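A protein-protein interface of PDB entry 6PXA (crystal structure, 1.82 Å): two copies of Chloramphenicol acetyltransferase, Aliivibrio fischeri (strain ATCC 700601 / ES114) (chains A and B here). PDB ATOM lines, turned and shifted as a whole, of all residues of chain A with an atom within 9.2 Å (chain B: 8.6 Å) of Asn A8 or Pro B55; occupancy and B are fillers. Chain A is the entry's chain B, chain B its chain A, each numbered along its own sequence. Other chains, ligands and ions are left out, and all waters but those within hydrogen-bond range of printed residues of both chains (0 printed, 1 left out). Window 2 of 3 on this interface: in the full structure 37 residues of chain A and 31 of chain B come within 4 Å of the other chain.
No position is printed for both chains.
Asn A8 touches just one residue of chain B: Pro B55.
Of chain A, only Asn A8, Ser A9, Trp A10 and Phe A36 come within 4 Å of Pro B55.
Ser A9 touches one residue of chain B.
Thr B56 touches two residues of chain A.
Of the printed residues of chain A, Leu B50 touches Trp A10 (3.6 Å).
Printed residues of chain B within 4 Å of Trp A10: Tyr B49 (3.3 Å), Leu B50 (3.6 Å), Leu B51 (3.6 Å), Asp B53 (2.7 Å), Pro B55 (3.7 Å) and Thr B56 (3.7 Å).
Printed residues of chain A within 4 Å of Glu B44: Tyr A37.
The side-chain carboxylate (OD2) of Asp B53 sits at hydrogen-bond distance from the indole nitrogen (NE1) of Trp A10 (2.7 Å).
N of Tyr B49 is in hydrogen-bond range of OH of Tyr A37 (2.9 Å).
The side-chain carboxylate (OD2) of Asp B53 sits at hydrogen-bond distance from the side-chain hydroxyl (OH) of Tyr A37 (3.5 Å).
Among the printed residues, pairs that only touch across the chains: Asn A8 with Pro B55 (3.7 Å), Ser A9 with Pro B55 (3.5 Å), Trp A10 with Tyr B49 (3.3 Å), Trp A10 with Leu B50 (3.6 Å), Trp A10 with Leu B51 (3.6 Å), Trp A10 with Pro B55 (3.7 Å), Trp A10 with Thr B56 (3.7 Å), Leu A11 with Thr B56 (3.7 Å), Phe A36 with Pro B55 (3.8 Å), Tyr A37 with Glu B44 (3.5 Å) and Tyr A37 with Val B47 (3.9 Å).
Hydrophobic or aromatic side chains of chain A that line the printed part of chain B: Trp A10, Leu A11, Phe A36 and Tyr A37.
Along chain A the printed residues that touch a printed residue of chain B span positions 8 to 37.
Of the 16 printed residues of chain B, 8 touch a printed residue of chain A.
Printed residues of chain B that touch a printed residue of chain A: Glu B44, Val B47, Tyr B49, Leu B50, Leu B51, Asp B53, Pro B55 and Thr B56.
Along chain B the printed residues that touch a printed residue of chain A span positions 44 to 56.
ND2 of Asn B22 sits close to N of Asp B53, 3.3 Å away.
OH of Tyr A37 lies close to NE1 of Trp A10, at 3.1 Å.
The backbone NH (N) of Ser A9 sits at hydrogen-bond distance from the side-chain carboxylate (OE1) of Glu A12, at 3.5 Å.
The backbone NH of Gly B52 is in hydrogen-bond range of the side-chain hydroxyl of Thr B56.
The backbone NH of Leu A11 sits close to the side-chain hydroxyl of Ser A9 (3.4 Å).
OG1 of Thr B56 lies within hydrogen-bond range of OD1 of Asp B53 (2.6 Å).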
ATOM      1  N   ALA A   3      11.296 -25.513   8.370  1.00  0.00           N
ATOM      2  CA  ALA A   3      11.552 -25.819   9.768  1.00  0.00           C
ATOM      3  C   ALA A   3      11.912 -24.557  10.538  1.00  0.00           C
ATOM      4  O   ALA A   3      12.627 -23.681  10.038  1.00  0.00           O
ATOM      5  CB  ALA A   3      12.675 -26.848   9.889  1.00  0.00           C
ATOM      6  N   MET A   4      11.416 -24.470  11.769  1.00  0.00           N
ATOM      7  CA  MET A   4      11.669 -23.286  12.563  1.00  0.00           C
ATOM      8  C   MET A   4      13.158 -23.146  12.850  1.00  0.00           C
ATOM      9  O   MET A   4      13.931 -24.105  12.765  1.00  0.00           O
ATOM     10  CB  MET A   4      10.892 -23.325  13.873  1.00  0.00           C
ATOM     11  CG  MET A   4      11.254 -24.464  14.782  1.00  0.00           C
ATOM     12  SD  MET A   4      10.468 -24.239  16.389  1.00  0.00           S
ATOM     13  CE  MET A   4      11.773 -23.389  17.282  1.00  0.00           C
ATOM     14  N   GLU A   5      13.547 -21.916  13.160  1.00  0.00           N
ATOM     15  CA  GLU A   5      14.883 -21.543  13.600  1.00  0.00           C
ATOM     16  C   GLU A   5      14.824 -21.048  15.039  1.00  0.00           C
ATOM     17  O   GLU A   5      13.753 -20.760  15.585  1.00  0.00           O
ATOM     18  CB  GLU A   5      15.486 -20.466  12.688  1.00  0.00           C
ATOM     19  CG  GLU A   5      15.329 -20.784  11.222  1.00  0.00           C
ATOM     20  CD  GLU A   5      16.356 -20.092  10.355  1.00  0.00           C
ATOM     21  OE1 GLU A   5      16.972 -19.105  10.826  1.00  0.00           O
ATOM     22  OE2 GLU A   5      16.546 -20.544   9.198  1.00  0.00           O
ATOM     23  N   ALA A   6      16.009 -20.935  15.646  1.00  0.00           N
ATOM     24  CA  ALA A   6      16.096 -20.673  17.079  1.00  0.00           C
ATOM     25  C   ALA A   6      15.773 -19.233  17.430  1.00  0.00           C
ATOM     26  O   ALA A   6      15.323 -18.961  18.550  1.00  0.00           O
ATOM     27  CB  ALA A   6      17.491 -21.027  17.596  1.00  0.00           C
ATOM     28  N   PHE A   7      15.995 -18.307  16.498  1.00  0.00           N
ATOM     29  CA  PHE A   7      15.826 -16.878  16.721  1.00  0.00           C
ATOM     30  C   PHE A   7      14.929 -16.282  15.640  1.00  0.00           C
ATOM     31  O   PHE A   7      15.008 -16.681  14.476  1.00  0.00           O
ATOM     32  CB  PHE A   7      17.178 -16.164  16.701  1.00  0.00           C
ATOM     33  CG  PHE A   7      18.119 -16.601  17.794  1.00  0.00           C
ATOM     34  CD1 PHE A   7      18.908 -17.716  17.635  1.00  0.00           C
ATOM     35  CD2 PHE A   7      18.215 -15.879  18.963  1.00  0.00           C
ATOM     36  CE1 PHE A   7      19.778 -18.100  18.618  1.00  0.00           C
ATOM     37  CE2 PHE A   7      19.079 -16.259  19.944  1.00  0.00           C
ATOM     38  CZ  PHE A   7      19.853 -17.380  19.771  1.00  0.00           C
ATOM     39  N   ASN A   8      14.088 -15.318  16.030  1.00  0.00           N
ATOM     40  CA  ASN A   8      13.182 -14.653  15.101  1.00  0.00           C
ATOM     41  C   ASN A   8      13.763 -13.377  14.510  1.00  0.00           C
ATOM     42  O   ASN A   8      13.355 -12.971  13.419  1.00  0.00           O
ATOM     43  CB  ASN A   8      11.855 -14.330  15.788  1.00  0.00           C
ATOM     44  CG  ASN A   8      10.972 -15.555  15.962  1.00  0.00           C
ATOM     45  OD1 ASN A   8      11.223 -16.610  15.372  1.00  0.00           O
ATOM     46  ND2 ASN A   8       9.920 -15.414  16.760  1.00  0.00           N
ATOM     47  N   SER A   9      14.694 -12.721  15.195  1.00  0.00           N
ATOM     48  CA  SER A   9      15.421 -11.621  14.574  1.00  0.00           C
ATOM     49  C   SER A   9      16.753 -11.489  15.286  1.00  0.00           C
ATOM     50  O   SER A   9      16.951 -12.047  16.368  1.00  0.00           O
ATOM     51  CB  SER A   9      14.637 -10.297  14.623  1.00  0.00           C
ATOM     52  OG  SER A   9      14.526  -9.818  15.948  1.00  0.00           O
ATOM     53  N   TRP A  10      17.672 -10.753  14.667  1.00  0.00           N
ATOM     54  CA  TRP A  10      18.956 -10.532  15.324  1.00  0.00           C
ATOM     55  C   TRP A  10      18.873  -9.519  16.449  1.00  0.00           C
ATOM     56  O   TRP A  10      19.896  -9.231  17.078  1.00  0.00           O
ATOM     57  CB  TRP A  10      20.023 -10.097  14.307  1.00  0.00           C
ATOM     58  CG  TRP A  10      19.583  -9.102  13.284  1.00  0.00           C
ATOM     59  CD1 TRP A  10      19.020  -9.373  12.056  1.00  0.00           C
ATOM     60  CD2 TRP A  10      19.695  -7.669  13.363  1.00  0.00           C
ATOM     61  NE1 TRP A  10      18.769  -8.195  11.377  1.00  0.00           N
ATOM     62  CE2 TRP A  10      19.180  -7.137  12.146  1.00  0.00           C
ATOM     63  CE3 TRP A  10      20.190  -6.787  14.328  1.00  0.00           C
ATOM     64  CZ2 TRP A  10      19.120  -5.753  11.888  1.00  0.00           C
ATOM     65  CZ3 TRP A  10      20.145  -5.425  14.071  1.00  0.00           C
ATOM     66  CH2 TRP A  10      19.612  -4.916  12.850  1.00  0.00           C
ATOM     67  N   LEU A  11      17.700  -8.944  16.696  1.00  0.00           N
ATOM     68  CA  LEU A  11      17.500  -8.103  17.860  1.00  0.00           C
ATOM     69  C   LEU A  11      17.408  -8.924  19.132  1.00  0.00           C
ATOM     70  O   LEU A  11      17.518  -8.362  20.223  1.00  0.00           O
ATOM     71  CB  LEU A  11      16.229  -7.264  17.707  1.00  0.00           C
ATOM     72  CG  LEU A  11      16.053  -6.342  16.485  1.00  0.00           C
ATOM     73  CD1 LEU A  11      14.799  -5.533  16.590  1.00  0.00           C
ATOM     74  CD2 LEU A  11      17.256  -5.431  16.272  1.00  0.00           C
ATOM     75  N   GLU A  12      17.236 -10.236  18.998  1.00  0.00           N
ATOM     76  CA  GLU A  12      16.953 -11.139  20.101  1.00  0.00           C
ATOM     77  C   GLU A  12      18.221 -11.830  20.569  1.00  0.00           C
ATOM     78  O   GLU A  12      19.019 -12.311  19.755  1.00  0.00           O
ATOM     79  CB  GLU A  12      15.943 -12.208  19.680  1.00  0.00           C
ATOM     80  CG  GLU A  12      14.540 -11.711  19.375  1.00  0.00           C
ATOM     81  CD  GLU A  12      13.596 -12.862  19.040  1.00  0.00           C
ATOM     82  OE1 GLU A  12      14.046 -13.838  18.397  1.00  0.00           O
ATOM     83  OE2 GLU A  12      12.414 -12.810  19.444  1.00  0.00           O
ATOM     84  N   GLY A  13      18.382 -11.906  21.891  1.00  0.00           N
ATOM     85  CA  GLY A  13      19.413 -12.724  22.486  1.00  0.00           C
ATOM     86  C   GLY A  13      18.812 -13.797  23.382  1.00  0.00           C
ATOM     87  O   GLY A  13      17.679 -13.650  23.854  1.00  0.00           O
ATOM     88  N   GLN A  14      19.556 -14.881  23.607  1.00  0.00           N
ATOM     89  CA  GLN A  14      19.123 -15.998  24.442  1.00  0.00           C
ATOM     90  C   GLN A  14      19.966 -16.029  25.710  1.00  0.00           C
ATOM     91  O   GLN A  14      21.173 -16.273  25.650  1.00  0.00           O
ATOM     92  CB  GLN A  14      19.245 -17.321  23.688  1.00  0.00           C
ATOM     93  CG  GLN A  14      17.933 -17.849  23.135  1.00  0.00           C
ATOM     94  CD  GLN A  14      17.019 -18.376  24.233  1.00  0.00           C
ATOM     95  OE1 GLN A  14      17.472 -18.685  25.335  1.00  0.00           O
ATOM     96  NE2 GLN A  14      15.730 -18.485  23.933  1.00  0.00           N
ATOM     97  N   GLY A  35      22.155 -15.502  18.212  1.00  0.00           N
ATOM     98  CA  GLY A  35      22.567 -16.455  17.202  1.00  0.00           C
ATOM     99  C   GLY A  35      21.713 -16.459  15.954  1.00  0.00           C
ATOM    100  O   GLY A  35      21.741 -17.439  15.210  1.00  0.00           O
ATOM    101  N   PHE A  36      20.978 -15.359  15.704  1.00  0.00           N
ATOM    102  CA  PHE A  36      20.032 -15.319  14.591  1.00  0.00           C
ATOM    103  C   PHE A  36      20.658 -15.770  13.273  1.00  0.00           C
ATOM    104  O   PHE A  36      20.046 -16.531  12.519  1.00  0.00           O
ATOM    105  CB  PHE A  36      19.460 -13.907  14.425  1.00  0.00           C
ATOM    106  CG  PHE A  36      18.592 -13.743  13.197  1.00  0.00           C
ATOM    107  CD1 PHE A  36      17.276 -14.196  13.191  1.00  0.00           C
ATOM    108  CD2 PHE A  36      19.089 -13.145  12.039  1.00  0.00           C
ATOM    109  CE1 PHE A  36      16.462 -14.042  12.043  1.00  0.00           C
ATOM    110  CE2 PHE A  36      18.285 -13.003  10.902  1.00  0.00           C
ATOM    111  CZ  PHE A  36      16.969 -13.461  10.912  1.00  0.00           C
ATOM    112  N   TYR A  37      21.854 -15.290  12.957  1.00  0.00           N
ATOM    113  CA  TYR A  37      22.348 -15.557  11.612  1.00  0.00           C
ATOM    114  C   TYR A  37      22.851 -16.986  11.424  1.00  0.00           C
ATOM    115  O   TYR A  37      23.121 -17.381  10.287  1.00  0.00           O
ATOM    116  CB  TYR A  37      23.436 -14.535  11.247  1.00  0.00           C
ATOM    117  CG  TYR A  37      22.816 -13.203  10.814  1.00  0.00           C
ATOM    118  CD1 TYR A  37      22.245 -13.055   9.545  1.00  0.00           C
ATOM    119  CD2 TYR A  37      22.759 -12.122  11.691  1.00  0.00           C
ATOM    120  CE1 TYR A  37      21.645 -11.825   9.156  1.00  0.00           C
ATOM    121  CE2 TYR A  37      22.158 -10.935  11.337  1.00  0.00           C
ATOM    122  CZ  TYR A  37      21.622 -10.787  10.068  1.00  0.00           C
ATOM    123  OH  TYR A  37      21.047  -9.598   9.749  1.00  0.00           O
ATOM    124  N   SER A  39      21.014 -19.700  12.943  1.00  0.00           N
ATOM    125  CA  SER A  39      19.771 -20.481  12.909  1.00  0.00           C
ATOM    126  C   SER A  39      19.486 -21.329  14.138  1.00  0.00           C
ATOM    127  O   SER A  39      18.316 -21.531  14.471  1.00  0.00           O
ATOM    128  CB  SER A  39      19.729 -21.394  11.681  1.00  0.00           C
ATOM    129  OG  SER A  39      19.740 -20.630  10.479  1.00  0.00           O
ATOM    130  N   ASN B  22      16.096  -3.091   0.710  1.00  0.00           N
ATOM    131  CA  ASN B  22      16.394  -2.350   1.929  1.00  0.00           C
ATOM    132  C   ASN B  22      16.716  -0.908   1.566  1.00  0.00           C
ATOM    133  O   ASN B  22      17.620  -0.677   0.755  1.00  0.00           O
ATOM    134  CB  ASN B  22      17.572  -3.006   2.659  1.00  0.00           C
ATOM    135  CG  ASN B  22      17.762  -2.496   4.080  1.00  0.00           C
ATOM    136  OD1 ASN B  22      17.529  -1.326   4.373  1.00  0.00           O
ATOM    137  ND2 ASN B  22      18.209  -3.383   4.969  1.00  0.00           N
ATOM    138  N   GLU B  43      20.370 -10.141   0.723  1.00  0.00           N
ATOM    139  CA  GLU B  43      19.860  -9.386   1.865  1.00  0.00           C
ATOM    140  C   GLU B  43      19.688 -10.252   3.117  1.00  0.00           C
ATOM    141  O   GLU B  43      19.760  -9.736   4.237  1.00  0.00           O
ATOM    142  CB  GLU B  43      18.531  -8.720   1.499  1.00  0.00           C
ATOM    143  CG  GLU B  43      18.668  -7.543   0.542  1.00  0.00           C
ATOM    144  CD  GLU B  43      17.425  -6.668   0.509  1.00  0.00           C
ATOM    145  OE1 GLU B  43      16.359  -7.106   0.005  1.00  0.00           O
ATOM    146  OE2 GLU B  43      17.524  -5.530   1.006  1.00  0.00           O
ATOM    147  N   GLU B  44      19.454 -11.552   2.966  1.00  0.00           N
ATOM    148  CA  GLU B  44      19.213 -12.375   4.149  1.00  0.00           C
ATOM    149  C   GLU B  44      20.496 -12.885   4.784  1.00  0.00           C
ATOM    150  O   GLU B  44      20.568 -13.039   6.009  1.00  0.00           O
ATOM    151  CB  GLU B  44      18.333 -13.572   3.798  1.00  0.00           C
ATOM    152  CG  GLU B  44      16.934 -13.210   3.441  1.00  0.00           C
ATOM    153  CD  GLU B  44      16.142 -14.427   3.030  1.00  0.00           C
ATOM    154  OE1 GLU B  44      16.720 -15.347   2.400  1.00  0.00           O
ATOM    155  OE2 GLU B  44      14.941 -14.463   3.350  1.00  0.00           O
ATOM    156  N   VAL B  47      24.276  -9.485   4.168  1.00  0.00           N
ATOM    157  CA  VAL B  47      24.216  -8.169   4.786  1.00  0.00           C
ATOM    158  C   VAL B  47      23.571  -8.363   6.143  1.00  0.00           C
ATOM    159  O   VAL B  47      22.394  -8.726   6.239  1.00  0.00           O
ATOM    160  CB  VAL B  47      23.436  -7.160   3.937  1.00  0.00           C
ATOM    161  CG1 VAL B  47      23.540  -5.742   4.579  1.00  0.00           C
ATOM    162  CG2 VAL B  47      23.970  -7.155   2.530  1.00  0.00           C
ATOM    163  N   TYR B  49      22.809  -7.385  10.293  1.00  0.00           N
ATOM    164  CA  TYR B  49      22.548  -6.359  11.317  1.00  0.00           C
ATOM    165  C   TYR B  49      22.210  -4.982  10.723  1.00  0.00           C
ATOM    166  O   TYR B  49      22.418  -3.949  11.372  1.00  0.00           O
ATOM    167  CB  TYR B  49      23.717  -6.243  12.301  1.00  0.00           C
ATOM    168  CG  TYR B  49      24.202  -7.604  12.778  1.00  0.00           C
ATOM    169  CD1 TYR B  49      23.556  -8.269  13.806  1.00  0.00           C
ATOM    170  CD2 TYR B  49      25.303  -8.223  12.185  1.00  0.00           C
ATOM    171  CE1 TYR B  49      23.988  -9.501  14.243  1.00  0.00           C
ATOM    172  CE2 TYR B  49      25.728  -9.470  12.602  1.00  0.00           C
ATOM    173  CZ  TYR B  49      25.075 -10.096  13.641  1.00  0.00           C
ATOM    174  OH  TYR B  49      25.491 -11.338  14.070  1.00  0.00           O
ATOM    175  N   LEU B  50      21.649  -4.932   9.511  1.00  0.00           N
ATOM    176  CA  LEU B  50      21.224  -3.664   8.901  1.00  0.00           C
ATOM    177  C   LEU B  50      19.736  -3.453   9.158  1.00  0.00           C
ATOM    178  O   LEU B  50      18.892  -4.183   8.626  1.00  0.00           O
ATOM    179  CB  LEU B  50      21.524  -3.653   7.400  1.00  0.00           C
ATOM    180  CG  LEU B  50      21.231  -2.322   6.728  1.00  0.00           C
ATOM    181  CD1 LEU B  50      22.085  -1.199   7.297  1.00  0.00           C
ATOM    182  CD2 LEU B  50      21.503  -2.483   5.246  1.00  0.00           C
ATOM    183  N   LEU B  51      19.409  -2.462   9.975  1.00  0.00           N
ATOM    184  CA  LEU B  51      18.010  -2.133  10.189  1.00  0.00           C
ATOM    185  C   LEU B  51      17.313  -1.882   8.853  1.00  0.00           C
ATOM    186  O   LEU B  51      17.897  -1.347   7.909  1.00  0.00           O
ATOM    187  CB  LEU B  51      17.898  -0.907  11.089  1.00  0.00           C
ATOM    188  CG  LEU B  51      18.280  -1.131  12.545  1.00  0.00           C
ATOM    189  CD1 LEU B  51      18.189   0.178  13.314  1.00  0.00           C
ATOM    190  CD2 LEU B  51      17.366  -2.183  13.175  1.00  0.00           C
ATOM    191  N   GLY B  52      16.054  -2.291   8.775  1.00  0.00           N
ATOM    192  CA  GLY B  52      15.303  -2.221   7.546  1.00  0.00           C
ATOM    193  C   GLY B  52      15.270  -3.510   6.752  1.00  0.00           C
ATOM    194  O   GLY B  52      14.567  -3.568   5.734  1.00  0.00           O
ATOM    195  N   ASP B  53      15.997  -4.540   7.189  1.00  0.00           N
ATOM    196  CA  ASP B  53      15.994  -5.834   6.523  1.00  0.00           C
ATOM    197  C   ASP B  53      14.709  -6.591   6.858  1.00  0.00           C
ATOM    198  O   ASP B  53      13.771  -6.056   7.457  1.00  0.00           O
ATOM    199  CB  ASP B  53      17.244  -6.632   6.902  1.00  0.00           C
ATOM    200  CG  ASP B  53      17.273  -7.089   8.399  1.00  0.00           C
ATOM    201  OD1 ASP B  53      16.375  -6.747   9.203  1.00  0.00           O
ATOM    202  OD2 ASP B  53      18.226  -7.821   8.762  1.00  0.00           O
ATOM    203  N   ALA B  54      14.666  -7.868   6.486  1.00  0.00           N
ATOM    204  CA  ALA B  54      13.444  -8.648   6.672  1.00  0.00           C
ATOM    205  C   ALA B  54      13.013  -8.735   8.133  1.00  0.00           C
ATOM    206  O   ALA B  54      11.879  -8.322   8.435  1.00  0.00           O
ATOM    207  CB  ALA B  54      13.610 -10.032   6.037  1.00  0.00           C
ATOM    208  N   PRO B  55      13.830  -9.222   9.082  1.00  0.00           N
ATOM    209  CA  PRO B  55      13.324  -9.379  10.456  1.00  0.00           C
ATOM    210  C   PRO B  55      13.150  -8.074  11.227  1.00  0.00           C
ATOM    211  O   PRO B  55      12.576  -8.112  12.324  1.00  0.00           O
ATOM    212  CB  PRO B  55      14.386 -10.272  11.122  1.00  0.00           C
ATOM    213  CG  PRO B  55      15.623  -9.942  10.420  1.00  0.00           C
ATOM    214  CD  PRO B  55      15.212  -9.738   8.977  1.00  0.00           C
ATOM    215  N   THR B  56      13.626  -6.928  10.720  1.00  0.00           N
ATOM    216  CA  THR B  56      13.477  -5.674  11.456  1.00  0.00           C
ATOM    217  C   THR B  56      12.767  -4.598  10.643  1.00  0.00           C
ATOM    218  O   THR B  56      12.853  -3.419  10.993  1.00  0.00           O
ATOM    219  CB  THR B  56      14.830  -5.127  11.922  1.00  0.00           C
ATOM    220  OG1 THR B  56      15.623  -4.786  10.776  1.00  0.00           O
ATOM    221  CG2 THR B  56      15.572  -6.148  12.789  1.00  0.00           C
ATOM    222  N   GLN B  57      12.077  -4.966   9.561  1.00  0.00           N
ATOM    223  CA  GLN B  57      11.412  -3.945   8.758  1.00  0.00           C
ATOM    224  C   GLN B  57      10.326  -3.237   9.557  1.00  0.00           C
ATOM    225  O   GLN B  57      10.145  -2.020   9.425  1.00  0.00           O
ATOM    226  CB  GLN B  57      10.832  -4.555   7.482  1.00  0.00           C
ATOM    227  CG  GLN B  57      10.128  -3.531   6.607  1.00  0.00           C
ATOM    228  CD  GLN B  57       9.564  -4.137   5.355  1.00  0.00           C
ATOM    229  OE1 GLN B  57       9.848  -5.292   5.036  1.00  0.00           O
ATOM    230  NE2 GLN B  57       8.753  -3.367   4.631  1.00  0.00           N
ATOM    231  N   GLU B  58       9.608  -3.977  10.408  1.00  0.00           N
ATOM    232  CA  GLU B  58       8.573  -3.369  11.241  1.00  0.00           C
ATOM    233  C   GLU B  58       9.154  -2.285  12.139  1.00  0.00           C
ATOM    234  O   GLU B  58       8.682  -1.143  12.136  1.00  0.00           O
ATOM    235  CB  GLU B  58       7.875  -4.438  12.086  1.00  0.00           C
ATOM    236  CG  GLU B  58       6.562  -4.949  11.513  1.00  0.00           C
ATOM    237  CD  GLU B  58       5.924  -6.022  12.384  1.00  0.00           C
ATOM    238  OE1 GLU B  58       4.775  -6.415  12.094  1.00  0.00           O
ATOM    239  OE2 GLU B  58       6.569  -6.473  13.355  1.00  0.00           O
ATOM    240  N   VAL B  59      10.190  -2.623  12.908  1.00  0.00           N
ATOM    241  CA  VAL B  59      10.714  -1.682  13.891  1.00  0.00           C
ATOM    242  C   VAL B  59      11.358  -0.482  13.206  1.00  0.00           C
ATOM    243  O   VAL B  59      11.288   0.645  13.715  1.00  0.00           O
ATOM    244  CB  VAL B  59      11.696  -2.396  14.840  1.00  0.00           C
ATOM    245  CG1 VAL B  59      11.749  -1.673  16.178  1.00  0.00           C
ATOM    246  CG2 VAL B  59      11.293  -3.853  15.036  1.00  0.00           C
ATOM    247  N   TRP B  60      11.982  -0.694  12.043  1.00  0.00           N
ATOM    248  CA  TRP B  60      12.581   0.415  11.303  1.00  0.00           C
ATOM    249  C   TRP B  60      11.520   1.369  10.761  1.00  0.00           C
ATOM    250  O   TRP B  60      11.677   2.594  10.845  1.00  0.00           O
ATOM    251  CB  TRP B  60      13.443  -0.127  10.167  1.00  0.00           C
ATOM    252  CG  TRP B  60      13.869   0.910   9.183  1.00  0.00           C
ATOM    253  CD1 TRP B  60      13.314   1.159   7.953  1.00  0.00           C
ATOM    254  CD2 TRP B  60      14.937   1.858   9.336  1.00  0.00           C
ATOM    255  NE1 TRP B  60      13.973   2.198   7.333  1.00  0.00           N
ATOM    256  CE2 TRP B  60      14.972   2.645   8.161  1.00  0.00           C
ATOM    257  CE3 TRP B  60      15.867   2.117  10.352  1.00  0.00           C
ATOM    258  CZ2 TRP B  60      15.903   3.670   7.974  1.00  0.00           C
ATOM    259  CZ3 TRP B  60      16.790   3.143  10.163  1.00  0.00           C
ATOM    260  CH2 TRP B  60      16.796   3.907   8.982  1.00  0.00           C
